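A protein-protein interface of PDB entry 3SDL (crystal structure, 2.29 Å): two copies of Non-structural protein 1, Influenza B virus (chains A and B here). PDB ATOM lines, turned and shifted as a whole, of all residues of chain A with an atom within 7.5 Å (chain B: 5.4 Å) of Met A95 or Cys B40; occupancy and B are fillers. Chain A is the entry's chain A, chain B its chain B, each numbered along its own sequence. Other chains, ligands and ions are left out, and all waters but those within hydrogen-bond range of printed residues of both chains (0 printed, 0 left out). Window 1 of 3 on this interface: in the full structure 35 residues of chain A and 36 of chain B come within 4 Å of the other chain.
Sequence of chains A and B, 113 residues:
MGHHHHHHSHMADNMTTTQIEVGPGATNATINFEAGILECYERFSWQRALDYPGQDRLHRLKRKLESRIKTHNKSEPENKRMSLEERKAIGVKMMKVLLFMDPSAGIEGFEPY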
ATOM      1  N   ASN A  32     -25.959  -5.105 -15.613  1.00  0.00           N
ATOM      2  CA  ASN A  32     -24.960  -6.044 -16.103  1.00  0.00           C
ATOM      3  C   ASN A  32     -24.179  -6.677 -14.964  1.00  0.00           C
ATOM      4  O   ASN A  32     -23.962  -7.889 -14.941  1.00  0.00           O
ATOM      5  CB  ASN A  32     -24.006  -5.351 -17.071  1.00  0.00           C
ATOM      6  CG  ASN A  32     -24.712  -4.832 -18.299  1.00  0.00           C
ATOM      7  OD1 ASN A  32     -25.649  -5.455 -18.793  1.00  0.00           O
ATOM      8  ND2 ASN A  32     -24.276  -3.680 -18.793  1.00  0.00           N
ATOM      9  N   PHE A  33     -23.760  -5.852 -14.015  1.00  0.00           N
ATOM     10  CA  PHE A  33     -23.072  -6.356 -12.842  1.00  0.00           C
ATOM     11  C   PHE A  33     -23.900  -7.440 -12.166  1.00  0.00           C
ATOM     12  O   PHE A  33     -23.398  -8.520 -11.862  1.00  0.00           O
ATOM     13  CB  PHE A  33     -22.805  -5.223 -11.856  1.00  0.00           C
ATOM     14  CG  PHE A  33     -22.312  -5.693 -10.530  1.00  0.00           C
ATOM     15  CD1 PHE A  33     -21.015  -6.157 -10.389  1.00  0.00           C
ATOM     16  CD2 PHE A  33     -23.141  -5.684  -9.426  1.00  0.00           C
ATOM     17  CE1 PHE A  33     -20.550  -6.596  -9.162  1.00  0.00           C
ATOM     18  CE2 PHE A  33     -22.684  -6.118  -8.198  1.00  0.00           C
ATOM     19  CZ  PHE A  33     -21.392  -6.580  -8.064  1.00  0.00           C
ATOM     20  N   GLU A  34     -25.177  -7.147 -11.943  1.00  0.00           N
ATOM     21  CA  GLU A  34     -26.046  -8.067 -11.226  1.00  0.00           C
ATOM     22  C   GLU A  34     -26.449  -9.261 -12.078  1.00  0.00           C
ATOM     23  O   GLU A  34     -26.849 -10.293 -11.551  1.00  0.00           O
ATOM     24  CB  GLU A  34     -27.270  -7.342 -10.681  1.00  0.00           C
ATOM     25  CG  GLU A  34     -26.939  -6.437  -9.509  1.00  0.00           C
ATOM     26  CD  GLU A  34     -28.162  -5.799  -8.910  1.00  0.00           C
ATOM     27  OE1 GLU A  34     -29.026  -5.348  -9.685  1.00  0.00           O
ATOM     28  OE2 GLU A  34     -28.262  -5.753  -7.668  1.00  0.00           O
ATOM     29  N   ALA A  35     -26.346  -9.119 -13.395  1.00  0.00           N
ATOM     30  CA  ALA A  35     -26.494 -10.266 -14.277  1.00  0.00           C
ATOM     31  C   ALA A  35     -25.394 -11.270 -13.943  1.00  0.00           C
ATOM     32  O   ALA A  35     -25.659 -12.454 -13.745  1.00  0.00           O
ATOM     33  CB  ALA A  35     -26.407  -9.843 -15.727  1.00  0.00           C
ATOM     34  N   GLY A  36     -24.162 -10.780 -13.871  1.00  0.00           N
ATOM     35  CA  GLY A  36     -23.027 -11.607 -13.505  1.00  0.00           C
ATOM     36  C   GLY A  36     -23.190 -12.224 -12.130  1.00  0.00           C
ATOM     37  O   GLY A  36     -22.758 -13.351 -11.894  1.00  0.00           O
ATOM     38  N   ILE A  37     -23.809 -11.480 -11.221  1.00  0.00           N
ATOM     39  CA  ILE A  37     -24.092 -11.975  -9.880  1.00  0.00           C
ATOM     40  C   ILE A  37     -24.989 -13.199  -9.967  1.00  0.00           C
ATOM     41  O   ILE A  37     -24.759 -14.204  -9.292  1.00  0.00           O
ATOM     42  CB  ILE A  37     -24.786 -10.899  -9.012  1.00  0.00           C
ATOM     43  CG1 ILE A  37     -23.828  -9.742  -8.725  1.00  0.00           C
ATOM     44  CG2 ILE A  37     -25.296 -11.501  -7.706  1.00  0.00           C
ATOM     45  CD1 ILE A  37     -22.589 -10.165  -7.966  1.00  0.00           C
ATOM     46  N   LEU A  38     -26.014 -13.105 -10.806  1.00  0.00           N
ATOM     47  CA  LEU A  38     -26.929 -14.214 -11.026  1.00  0.00           C
ATOM     48  C   LEU A  38     -26.191 -15.429 -11.575  1.00  0.00           C
ATOM     49  O   LEU A  38     -26.418 -16.560 -11.142  1.00  0.00           O
ATOM     50  CB  LEU A  38     -28.033 -13.801 -11.998  1.00  0.00           C
ATOM     51  CG  LEU A  38     -29.009 -14.906 -12.394  1.00  0.00           C
ATOM     52  CD1 LEU A  38     -29.784 -15.379 -11.179  1.00  0.00           C
ATOM     53  CD2 LEU A  38     -29.955 -14.417 -13.481  1.00  0.00           C
ATOM     54  N   GLU A  39     -25.305 -15.185 -12.533  1.00  0.00           N
ATOM     55  CA  GLU A  39     -24.535 -16.251 -13.155  1.00  0.00           C
ATOM     56  C   GLU A  39     -23.684 -16.989 -12.129  1.00  0.00           C
ATOM     57  O   GLU A  39     -23.444 -18.186 -12.264  1.00  0.00           O
ATOM     58  CB  GLU A  39     -23.659 -15.691 -14.277  1.00  0.00           C
ATOM     59  CG  GLU A  39     -22.747 -16.712 -14.937  1.00  0.00           C
ATOM     60  CD  GLU A  39     -23.507 -17.810 -15.653  1.00  0.00           C
ATOM     61  OE1 GLU A  39     -24.718 -17.640 -15.904  1.00  0.00           O
ATOM     62  OE2 GLU A  39     -22.887 -18.848 -15.963  1.00  0.00           O
ATOM     63  N   CYS A  40     -23.230 -16.274 -11.104  1.00  0.00           N
ATOM     64  CA  CYS A  40     -22.452 -16.891 -10.035  1.00  0.00           C
ATOM     65  C   CYS A  40     -23.353 -17.694  -9.104  1.00  0.00           C
ATOM     66  O   CYS A  40     -23.017 -18.813  -8.724  1.00  0.00           O
ATOM     67  CB  CYS A  40     -21.666 -15.839  -9.247  1.00  0.00           C
ATOM     68  SG  CYS A  40     -20.392 -14.983 -10.205  1.00  0.00           S
ATOM     69  N   TYR A  41     -24.496 -17.122  -8.734  1.00  0.00           N
ATOM     70  CA  TYR A  41     -25.472 -17.856  -7.935  1.00  0.00           C
ATOM     71  C   TYR A  41     -25.769 -19.190  -8.602  1.00  0.00           C
ATOM     72  O   TYR A  41     -25.719 -20.239  -7.962  1.00  0.00           O
ATOM     73  CB  TYR A  41     -26.769 -17.061  -7.760  1.00  0.00           C
ATOM     74  CG  TYR A  41     -26.826 -16.262  -6.475  1.00  0.00           C
ATOM     75  CD1 TYR A  41     -26.258 -14.994  -6.394  1.00  0.00           C
ATOM     76  CD2 TYR A  41     -27.449 -16.774  -5.344  1.00  0.00           C
ATOM     77  CE1 TYR A  41     -26.303 -14.261  -5.222  1.00  0.00           C
ATOM     78  CE2 TYR A  41     -27.500 -16.047  -4.164  1.00  0.00           C
ATOM     79  CZ  TYR A  41     -26.925 -14.790  -4.111  1.00  0.00           C
ATOM     80  OH  TYR A  41     -26.972 -14.059  -2.944  1.00  0.00           O
ATOM     81  N   ALA A  89     -22.229 -12.207 -19.639  1.00  0.00           N
ATOM     82  CA  ALA A  89     -20.840 -12.226 -20.080  1.00  0.00           C
ATOM     83  C   ALA A  89     -20.107 -10.956 -19.661  1.00  0.00           C
ATOM     84  O   ALA A  89     -18.959 -11.007 -19.219  1.00  0.00           O
ATOM     85  CB  ALA A  89     -20.769 -12.411 -21.587  1.00  0.00           C
ATOM     86  N   ILE A  90     -20.777  -9.815 -19.802  1.00  0.00           N
ATOM     87  CA  ILE A  90     -20.186  -8.536 -19.421  1.00  0.00           C
ATOM     88  C   ILE A  90     -20.003  -8.455 -17.909  1.00  0.00           C
ATOM     89  O   ILE A  90     -18.970  -7.993 -17.423  1.00  0.00           O
ATOM     90  CB  ILE A  90     -21.039  -7.355 -19.907  1.00  0.00           C
ATOM     91  CG1 ILE A  90     -21.099  -7.339 -21.435  1.00  0.00           C
ATOM     92  CG2 ILE A  90     -20.472  -6.044 -19.391  1.00  0.00           C
ATOM     93  CD1 ILE A  90     -22.104  -6.360 -21.993  1.00  0.00           C
ATOM     94  N   GLY A  91     -21.006  -8.921 -17.170  1.00  0.00           N
ATOM     95  CA  GLY A  91     -20.949  -8.916 -15.719  1.00  0.00           C
ATOM     96  C   GLY A  91     -19.867  -9.823 -15.162  1.00  0.00           C
ATOM     97  O   GLY A  91     -19.237  -9.500 -14.159  1.00  0.00           O
ATOM     98  N   VAL A  92     -19.653 -10.966 -15.809  1.00  0.00           N
ATOM     99  CA  VAL A  92     -18.602 -11.891 -15.394  1.00  0.00           C
ATOM    100  C   VAL A  92     -17.233 -11.224 -15.455  1.00  0.00           C
ATOM    101  O   VAL A  92     -16.462 -11.265 -14.491  1.00  0.00           O
ATOM    102  CB  VAL A  92     -18.567 -13.162 -16.271  1.00  0.00           C
ATOM    103  CG1 VAL A  92     -17.331 -13.988 -15.948  1.00  0.00           C
ATOM    104  CG2 VAL A  92     -19.833 -13.987 -16.081  1.00  0.00           C
ATOM    105  N   LYS A  93     -16.936 -10.612 -16.595  1.00  0.00           N
ATOM    106  CA  LYS A  93     -15.668  -9.918 -16.779  1.00  0.00           C
ATOM    107  C   LYS A  93     -15.495  -8.833 -15.729  1.00  0.00           C
ATOM    108  O   LYS A  93     -14.419  -8.685 -15.150  1.00  0.00           O
ATOM    109  CB  LYS A  93     -15.584  -9.323 -18.183  1.00  0.00           C
ATOM    110  CG  LYS A  93     -15.472 -10.369 -19.278  1.00  0.00           C
ATOM    111  CD  LYS A  93     -16.243  -9.963 -20.521  1.00  0.00           C
ATOM    112  CE  LYS A  93     -16.114 -11.006 -21.622  1.00  0.00           C
ATOM    113  NZ  LYS A  93     -16.952 -10.677 -22.810  1.00  0.00           N
ATOM    114  N   MET A  94     -16.563  -8.080 -15.478  1.00  0.00           N
ATOM    115  CA  MET A  94     -16.521  -7.024 -14.476  1.00  0.00           C
ATOM    116  C   MET A  94     -16.182  -7.592 -13.103  1.00  0.00           C
ATOM    117  O   MET A  94     -15.356  -7.037 -12.381  1.00  0.00           O
ATOM    118  CB  MET A  94     -17.840  -6.237 -14.432  1.00  0.00           C
ATOM    119  CG  MET A  94     -18.098  -5.377 -15.661  1.00  0.00           C
ATOM    120  SD  MET A  94     -19.322  -4.072 -15.426  1.00  0.00           S
ATOM    121  CE  MET A  94     -20.768  -5.025 -14.982  1.00  0.00           C
ATOM    122  N   MET A  95     -16.810  -8.707 -12.745  1.00  0.00           N
ATOM    123  CA  MET A  95     -16.556  -9.316 -11.443  1.00  0.00           C
ATOM    124  C   MET A  95     -15.126  -9.829 -11.312  1.00  0.00           C
ATOM    125  O   MET A  95     -14.513  -9.714 -10.249  1.00  0.00           O
ATOM    126  CB  MET A  95     -17.556 -10.431 -11.150  1.00  0.00           C
ATOM    127  CG  MET A  95     -18.855  -9.948 -10.524  1.00  0.00           C
ATOM    128  SD  MET A  95     -19.925 -11.329 -10.077  1.00  0.00           S
ATOM    129  CE  MET A  95     -18.975 -12.089  -8.765  1.00  0.00           C
ATOM    130  N   LYS A  96     -14.595 -10.392 -12.394  1.00  0.00           N
ATOM    131  CA  LYS A  96     -13.213 -10.862 -12.395  1.00  0.00           C
ATOM    132  C   LYS A  96     -12.248  -9.710 -12.116  1.00  0.00           C
ATOM    133  O   LYS A  96     -11.264  -9.868 -11.392  1.00  0.00           O
ATOM    134  CB  LYS A  96     -12.866 -11.527 -13.727  1.00  0.00           C
ATOM    135  CG  LYS A  96     -13.597 -12.834 -14.001  1.00  0.00           C
ATOM    136  CD  LYS A  96     -13.148 -13.420 -15.334  1.00  0.00           C
ATOM    137  CE  LYS A  96     -13.903 -14.696 -15.677  1.00  0.00           C
ATOM    138  NZ  LYS A  96     -13.459 -15.254 -16.986  1.00  0.00           N
ATOM    139  N   VAL A  97     -12.531  -8.547 -12.688  1.00  0.00           N
ATOM    140  CA  VAL A  97     -11.680  -7.384 -12.458  1.00  0.00           C
ATOM    141  C   VAL A  97     -11.719  -6.941 -11.001  1.00  0.00           C
ATOM    142  O   VAL A  97     -10.704  -6.538 -10.447  1.00  0.00           O
ATOM    143  CB  VAL A  97     -12.058  -6.193 -13.360  1.00  0.00           C
ATOM    144  CG1 VAL A  97     -11.131  -5.022 -13.094  1.00  0.00           C
ATOM    145  CG2 VAL A  97     -11.993  -6.594 -14.817  1.00  0.00           C
ATOM    146  N   LEU A  98     -12.891  -7.015 -10.380  1.00  0.00           N
ATOM    147  CA  LEU A  98     -13.036  -6.555  -9.000  1.00  0.00           C
ATOM    148  C   LEU A  98     -12.383  -7.527  -8.022  1.00  0.00           C
ATOM    149  O   LEU A  98     -11.746  -7.119  -7.051  1.00  0.00           O
ATOM    150  CB  LEU A  98     -14.512  -6.365  -8.646  1.00  0.00           C
ATOM    151  CG  LEU A  98     -15.260  -5.272  -9.415  1.00  0.00           C
ATOM    152  CD1 LEU A  98     -16.745  -5.308  -9.100  1.00  0.00           C
ATOM    153  CD2 LEU A  98     -14.676  -3.905  -9.103  1.00  0.00           C
ATOM    154  N   LEU A  99     -12.549  -8.820  -8.281  1.00  0.00           N
ATOM    155  CA  LEU A  99     -11.980  -9.845  -7.418  1.00  0.00           C
ATOM    156  C   LEU A  99     -10.459  -9.882  -7.517  1.00  0.00           C
ATOM    157  O   LEU A  99      -9.764  -9.978  -6.508  1.00  0.00           O
ATOM    158  CB  LEU A  99     -12.574 -11.213  -7.752  1.00  0.00           C
ATOM    159  CG  LEU A  99     -14.046 -11.359  -7.370  1.00  0.00           C
ATOM    160  CD1 LEU A  99     -14.553 -12.743  -7.705  1.00  0.00           C
ATOM    161  CD2 LEU A  99     -14.241 -11.055  -5.891  1.00  0.00           C
ATOM    162  N   PHE A 100      -9.943  -9.798  -8.737  1.00  0.00           N
ATOM    163  CA  PHE A 100      -8.501  -9.820  -8.939  1.00  0.00           C
ATOM    164  C   PHE A 100      -7.905  -8.422  -8.935  1.00  0.00           C
ATOM    165  O   PHE A 100      -6.683  -8.262  -8.920  1.00  0.00           O
ATOM    166  CB  PHE A 100      -8.154 -10.534 -10.241  1.00  0.00           C
ATOM    167  CG  PHE A 100      -8.455 -11.999 -10.215  1.00  0.00           C
ATOM    168  CD1 PHE A 100      -7.547 -12.893  -9.674  1.00  0.00           C
ATOM    169  CD2 PHE A 100      -9.651 -12.484 -10.713  1.00  0.00           C
ATOM    170  CE1 PHE A 100      -7.823 -14.245  -9.638  1.00  0.00           C
ATOM    171  CE2 PHE A 100      -9.931 -13.836 -10.677  1.00  0.00           C
ATOM    172  CZ  PHE A 100      -9.013 -14.716 -10.142  1.00  0.00           C
ATOM    173  N   MET A 101      -8.768  -7.411  -8.938  1.00  0.00           N
ATOM    174  CA  MET A 101      -8.310  -6.028  -8.982  1.00  0.00           C
ATOM    175  C   MET A 101      -7.282  -5.860 -10.089  1.00  0.00           C
ATOM    176  O   MET A 101      -6.165  -5.406  -9.850  1.00  0.00           O
ATOM    177  CB  MET A 101      -7.715  -5.619  -7.636  1.00  0.00           C
ATOM    178  CG  MET A 101      -8.736  -5.573  -6.512  1.00  0.00           C
ATOM    179  SD  MET A 101     -10.066  -4.403  -6.854  1.00  0.00           S
ATOM    180  CE  MET A 101      -9.139  -2.880  -6.986  1.00  0.00           C
ATOM    181  N   ALA A 105      -8.440  -8.991 -16.581  1.00  0.00           N
ATOM    182  CA  ALA A 105      -9.411 -10.078 -16.437  1.00  0.00           C
ATOM    183  C   ALA A 105     -10.392 -10.265 -17.610  1.00  0.00           C
ATOM    184  O   ALA A 105     -10.569 -11.386 -18.086  1.00  0.00           O
ATOM    185  CB  ALA A 105     -10.160  -9.950 -15.116  1.00  0.00           C
ATOM    186  N   GLY A 109     -14.793  -5.442 -19.386  1.00  0.00           N
ATOM    187  CA  GLY A 109     -15.499  -4.674 -18.377  1.00  0.00           C
ATOM    188  C   GLY A 109     -15.132  -3.204 -18.459  1.00  0.00           C
ATOM    189  O   GLY A 109     -15.604  -2.390 -17.665  1.00  0.00           O
ATOM    190  N   GLY B  36     -19.010 -13.233  -0.191  1.00  0.00           N
ATOM    191  CA  GLY B  36     -18.165 -12.850  -1.307  1.00  0.00           C
ATOM    192  C   GLY B  36     -18.928 -12.015  -2.317  1.00  0.00           C
ATOM    193  O   GLY B  36     -18.358 -11.152  -2.986  1.00  0.00           O
ATOM    194  N   ILE B  37     -20.226 -12.276  -2.426  1.00  0.00           N
ATOM    195  CA  ILE B  37     -21.098 -11.493  -3.289  1.00  0.00           C
ATOM    196  C   ILE B  37     -21.148 -10.059  -2.772  1.00  0.00           C
ATOM    197  O   ILE B  37     -21.114  -9.100  -3.549  1.00  0.00           O
ATOM    198  CB  ILE B  37     -22.524 -12.084  -3.330  1.00  0.00           C
ATOM    199  CG1 ILE B  37     -22.530 -13.430  -4.066  1.00  0.00           C
ATOM    200  CG2 ILE B  37     -23.489 -11.124  -4.000  1.00  0.00           C
ATOM    201  CD1 ILE B  37     -22.217 -13.331  -5.549  1.00  0.00           C
ATOM    202  N   LEU B  38     -21.213  -9.919  -1.452  1.00  0.00           N
ATOM    203  CA  LEU B  38     -21.216  -8.606  -0.821  1.00  0.00           C
ATOM    204  C   LEU B  38     -19.913  -7.865  -1.105  1.00  0.00           C
ATOM    205  O   LEU B  38     -19.919  -6.673  -1.407  1.00  0.00           O
ATOM    206  CB  LEU B  38     -21.425  -8.729   0.689  1.00  0.00           C
ATOM    207  CG  LEU B  38     -21.422  -7.409   1.462  1.00  0.00           C
ATOM    208  CD1 LEU B  38     -22.575  -6.519   1.007  1.00  0.00           C
ATOM    209  CD2 LEU B  38     -21.487  -7.652   2.959  1.00  0.00           C
ATOM    210  N   GLU B  39     -18.794  -8.574  -0.998  1.00  0.00           N
ATOM    211  CA  GLU B  39     -17.491  -7.976  -1.262  1.00  0.00           C
ATOM    212  C   GLU B  39     -17.433  -7.444  -2.691  1.00  0.00           C
ATOM    213  O   GLU B  39     -16.720  -6.485  -2.979  1.00  0.00           O
ATOM    214  CB  GLU B  39     -16.370  -8.993  -1.025  1.00  0.00           C
ATOM    215  CG  GLU B  39     -14.965  -8.463  -1.296  1.00  0.00           C
ATOM    216  CD  GLU B  39     -14.559  -7.339  -0.352  1.00  0.00           C
ATOM    217  OE1 GLU B  39     -15.299  -7.065   0.617  1.00  0.00           O
ATOM    218  OE2 GLU B  39     -13.496  -6.727  -0.581  1.00  0.00           O
ATOM    219  N   CYS B  40     -18.184  -8.082  -3.584  1.00  0.00           N
ATOM    220  CA  CYS B  40     -18.221  -7.680  -4.984  1.00  0.00           C
ATOM    221  C   CYS B  40     -19.133  -6.474  -5.174  1.00  0.00           C
ATOM    222  O   CYS B  40     -18.847  -5.591  -5.982  1.00  0.00           O
ATOM    223  CB  CYS B  40     -18.684  -8.841  -5.868  1.00  0.00           C
ATOM    224  SG  CYS B  40     -17.524 -10.224  -5.974  1.00  0.00           S
ATOM    225  N   TYR B  41     -20.237  -6.444  -4.433  1.00  0.00           N
ATOM    226  CA  TYR B  41     -21.133  -5.298  -4.449  1.00  0.00           C
ATOM    227  C   TYR B  41     -20.393  -4.053  -3.987  1.00  0.00           C
ATOM    228  O   TYR B  41     -20.410  -3.026  -4.662  1.00  0.00           O
ATOM    229  CB  TYR B  41     -22.361  -5.546  -3.571  1.00  0.00           C
ATOM    230  CG  TYR B  41     -23.553  -6.070  -4.339  1.00  0.00           C
ATOM    231  CD1 TYR B  41     -23.741  -7.432  -4.522  1.00  0.00           C
ATOM    232  CD2 TYR B  41     -24.485  -5.201  -4.886  1.00  0.00           C
ATOM    233  CE1 TYR B  41     -24.825  -7.915  -5.227  1.00  0.00           C
ATOM    234  CE2 TYR B  41     -25.575  -5.674  -5.594  1.00  0.00           C
ATOM    235  CZ  TYR B  41     -25.739  -7.032  -5.761  1.00  0.00           C
ATOM    236  OH  TYR B  41     -26.819  -7.513  -6.464  1.00  0.00           O
ATOM    237  N   GLU B  42     -19.728  -4.164  -2.840  1.00  0.00           N
ATOM    238  CA  GLU B  42     -18.958  -3.059  -2.276  1.00  0.00           C
ATOM    239  C   GLU B  42     -17.880  -2.546  -3.229  1.00  0.00           C
ATOM    240  O   GLU B  42     -17.806  -1.347  -3.506  1.00  0.00           O
ATOM    241  CB  GLU B  42     -18.323  -3.477  -0.950  1.00  0.00           C
ATOM    242  CG  GLU B  42     -19.333  -3.863   0.121  1.00  0.00           C
ATOM    243  CD  GLU B  42     -18.684  -4.149   1.458  1.00  0.00           C
ATOM    244  OE1 GLU B  42     -17.440  -4.217   1.515  1.00  0.00           O
ATOM    245  OE2 GLU B  42     -19.419  -4.299   2.455  1.00  0.00           O
ATOM    246  N   ARG B  43     -17.045  -3.457  -3.720  1.00  0.00           N
ATOM    247  CA  ARG B  43     -15.978  -3.098  -4.645  1.00  0.00           C
ATOM    248  C   ARG B  43     -16.540  -2.455  -5.908  1.00  0.00           C
ATOM    249  O   ARG B  43     -15.955  -1.517  -6.446  1.00  0.00           O
ATOM    250  CB  ARG B  43     -15.135  -4.325  -5.002  1.00  0.00           C
ATOM    251  CG  ARG B  43     -14.315  -4.875  -3.841  1.00  0.00           C
ATOM    252  CD  ARG B  43     -13.952  -6.328  -4.069  1.00  0.00           C
ATOM    253  NE  ARG B  43     -12.570  -6.503  -4.496  1.00  0.00           N
ATOM    254  CZ  ARG B  43     -11.688  -7.263  -3.856  1.00  0.00           C
ATOM    255  NH1 ARG B  43     -12.043  -7.916  -2.760  1.00  0.00           N
ATOM    256  NH2 ARG B  43     -10.449  -7.372  -4.314  1.00  0.00           N
ATOM    257  N   PHE B  44     -17.671  -2.963  -6.384  1.00  0.00           N
ATOM    258  CA  PHE B  44     -18.336  -2.364  -7.535  1.00  0.00           C
ATOM    259  C   PHE B  44     -18.793  -0.954  -7.177  1.00  0.00           C
ATOM    260  O   PHE B  44     -18.670  -0.024  -7.977  1.00  0.00           O
ATOM    261  CB  PHE B  44     -19.527  -3.221  -7.963  1.00  0.00           C
ATOM    262  CG  PHE B  44     -20.125  -2.827  -9.289  1.00  0.00           C
ATOM    263  CD1 PHE B  44     -19.370  -2.878 -10.448  1.00  0.00           C
ATOM    264  CD2 PHE B  44     -21.450  -2.447  -9.378  1.00  0.00           C
ATOM    265  CE1 PHE B  44     -19.919  -2.531 -11.670  1.00  0.00           C
ATOM    266  CE2 PHE B  44     -22.009  -2.101 -10.598  1.00  0.00           C
ATOM    267  CZ  PHE B  44     -21.240  -2.147 -11.746  1.00  0.00           C
ATOM    268  N   SER B  45     -19.297  -0.797  -5.957  1.00  0.00           N
ATOM    269  CA  SER B  45     -19.838   0.481  -5.507  1.00  0.00           C
ATOM    270  C   SER B  45     -18.810   1.609  -5.563  1.00  0.00           C
ATOM    271  O   SER B  45     -19.159   2.759  -5.811  1.00  0.00           O
ATOM    272  CB  SER B  45     -20.395   0.356  -4.093  1.00  0.00           C
ATOM    273  OG  SER B  45     -21.114   1.520  -3.733  1.00  0.00           O
ATOM    274  N   MET B  95     -15.858 -17.494  -5.498  1.00  0.00           N
ATOM    275  CA  MET B  95     -16.262 -16.706  -6.648  1.00  0.00           C
ATOM    276  C   MET B  95     -15.245 -16.854  -7.767  1.00  0.00           C
ATOM    277  O   MET B  95     -15.603 -16.966  -8.940  1.00  0.00           O
ATOM    278  CB  MET B  95     -16.394 -15.238  -6.256  1.00  0.00           C
ATOM    279  CG  MET B  95     -17.590 -14.553  -6.866  1.00  0.00           C
ATOM    280  SD  MET B  95     -19.118 -15.222  -6.193  1.00  0.00           S
ATOM    281  CE  MET B  95     -18.986 -14.676  -4.494  1.00  0.00           C
ATOM    282  N   LEU B  99     -16.233 -18.226 -11.343  1.00  0.00           N
ATOM    283  CA  LEU B  99     -16.111 -17.354 -12.506  1.00  0.00           C
ATOM    284  C   LEU B  99     -15.299 -18.008 -13.624  1.00  0.00           C
ATOM    285  O   LEU B  99     -15.580 -17.815 -14.810  1.00  0.00           O
ATOM    286  CB  LEU B  99     -15.494 -16.012 -12.104  1.00  0.00           C
ATOM    287  CG  LEU B  99     -16.407 -15.058 -11.329  1.00  0.00           C
ATOM    288  CD1 LEU B  99     -15.621 -13.877 -10.799  1.00  0.00           C
ATOM    289  CD2 LEU B  99     -17.538 -14.587 -12.216  1.00  0.00           C
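The side-chain carboxylate (OE2) of Glu A34 lies within hydrogen-bond range of the side-chain hydroxyl (OH) of Tyr B41. O of Leu A98 lies within hydrogen-bond range of NE of Arg B43. The backbone carbonyl oxygen of Leu A99 lies within hydrogen-bond range of the guanidinium group of Arg B43, 3.5 Å away.
The side-chain sulfur (SG) of Cys A40 lies within hydrogen-bond range of the backbone carbonyl oxygen (O) of Gly A36 (3.3 Å). The side-chain sulfur of Met A95 sits close to the side-chain sulfur of Cys A40 (3.7 Å). O of Gly B36 sits at hydrogen-bond distance from SG of Cys B40 (3.2 Å). NH1 of Arg B43 lies within salt-bridge range of OE2 of Glu B39, 2.9 Å away.
Among the printed residues, merely in contact across the chains: Phe A33 with Cys B40 (3.4 Å), Phe A33 with Tyr B41 (3.8 Å), Phe A33 with Phe B44 (3.5 Å), Cys A40 with Leu B99 (3.5 Å), Val A92 with Leu B99 (3.8 Å), Met A95 with Cys B40 (3.7 Å), Met A95 with Met B95 (3.4 Å), Met A95 with Leu B99 (3.97 Å), Lys A96 with Leu B99 (3.6 Å), Leu A98 with Cys B40 (3.8 Å), Leu A98 with Phe B44 (3.7 Å), Leu A99 with Cys B40 (3.4 Å), Leu A99 with Met B95 (3.4 Å), Leu A99 with Leu B99 (3.5 Å) and Met A101 with Arg B43 (3.3 Å).
Of chain B, only Cys B40 (3.7 Å), Met B95 (3.4 Å) and Leu B99 (3.97 Å) come within 4 Å of Met A95. Of chain A, only Phe A33 (3.4 Å), Met A95 (3.7 Å), Leu A98 (3.8 Å) and Leu A99 (3.4 Å) come within 4 Å of Cys B40. Of the printed residues of chain B, Glu A34 touches Tyr B41. Printed residues of chain A within 4 Å of Tyr B41: Phe A33 (3.8 Å) and Glu A34 (2.6 Å). Gly B36 touches none of the printed residues of chain A. Ile B37 touches none of the printed residues of chain A.
Of the 25 printed residues of chain A, 9 touch a printed residue of chain B. Printed residues of chain A that touch a printed residue of chain B: Phe A33, Glu A34, Cys A40, Val A92, Met A95, Lys A96, Leu A98, Leu A99 and Met A101. Hydrophobic or aromatic side chains of chain B within 4 Å of the printed part of chain A: Tyr B41, Phe B44, Met B95 and Leu B99.
Cys A40 touches Leu B99, and with the chains exchanged Leu A99 touches Cys B40. Met A95 touches Cys B40, but with the chains exchanged Cys A40 does not touch Met B95 (4.02 Å). Met A95 touches Leu B99, and with the chains exchanged Leu A99 touches Met B95. Leu B99 touches its own counterpart, Leu A99. Of the 18 pairs that touch across the chains among the printed residues, 6 have their exchanged pair printed and touching as well.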
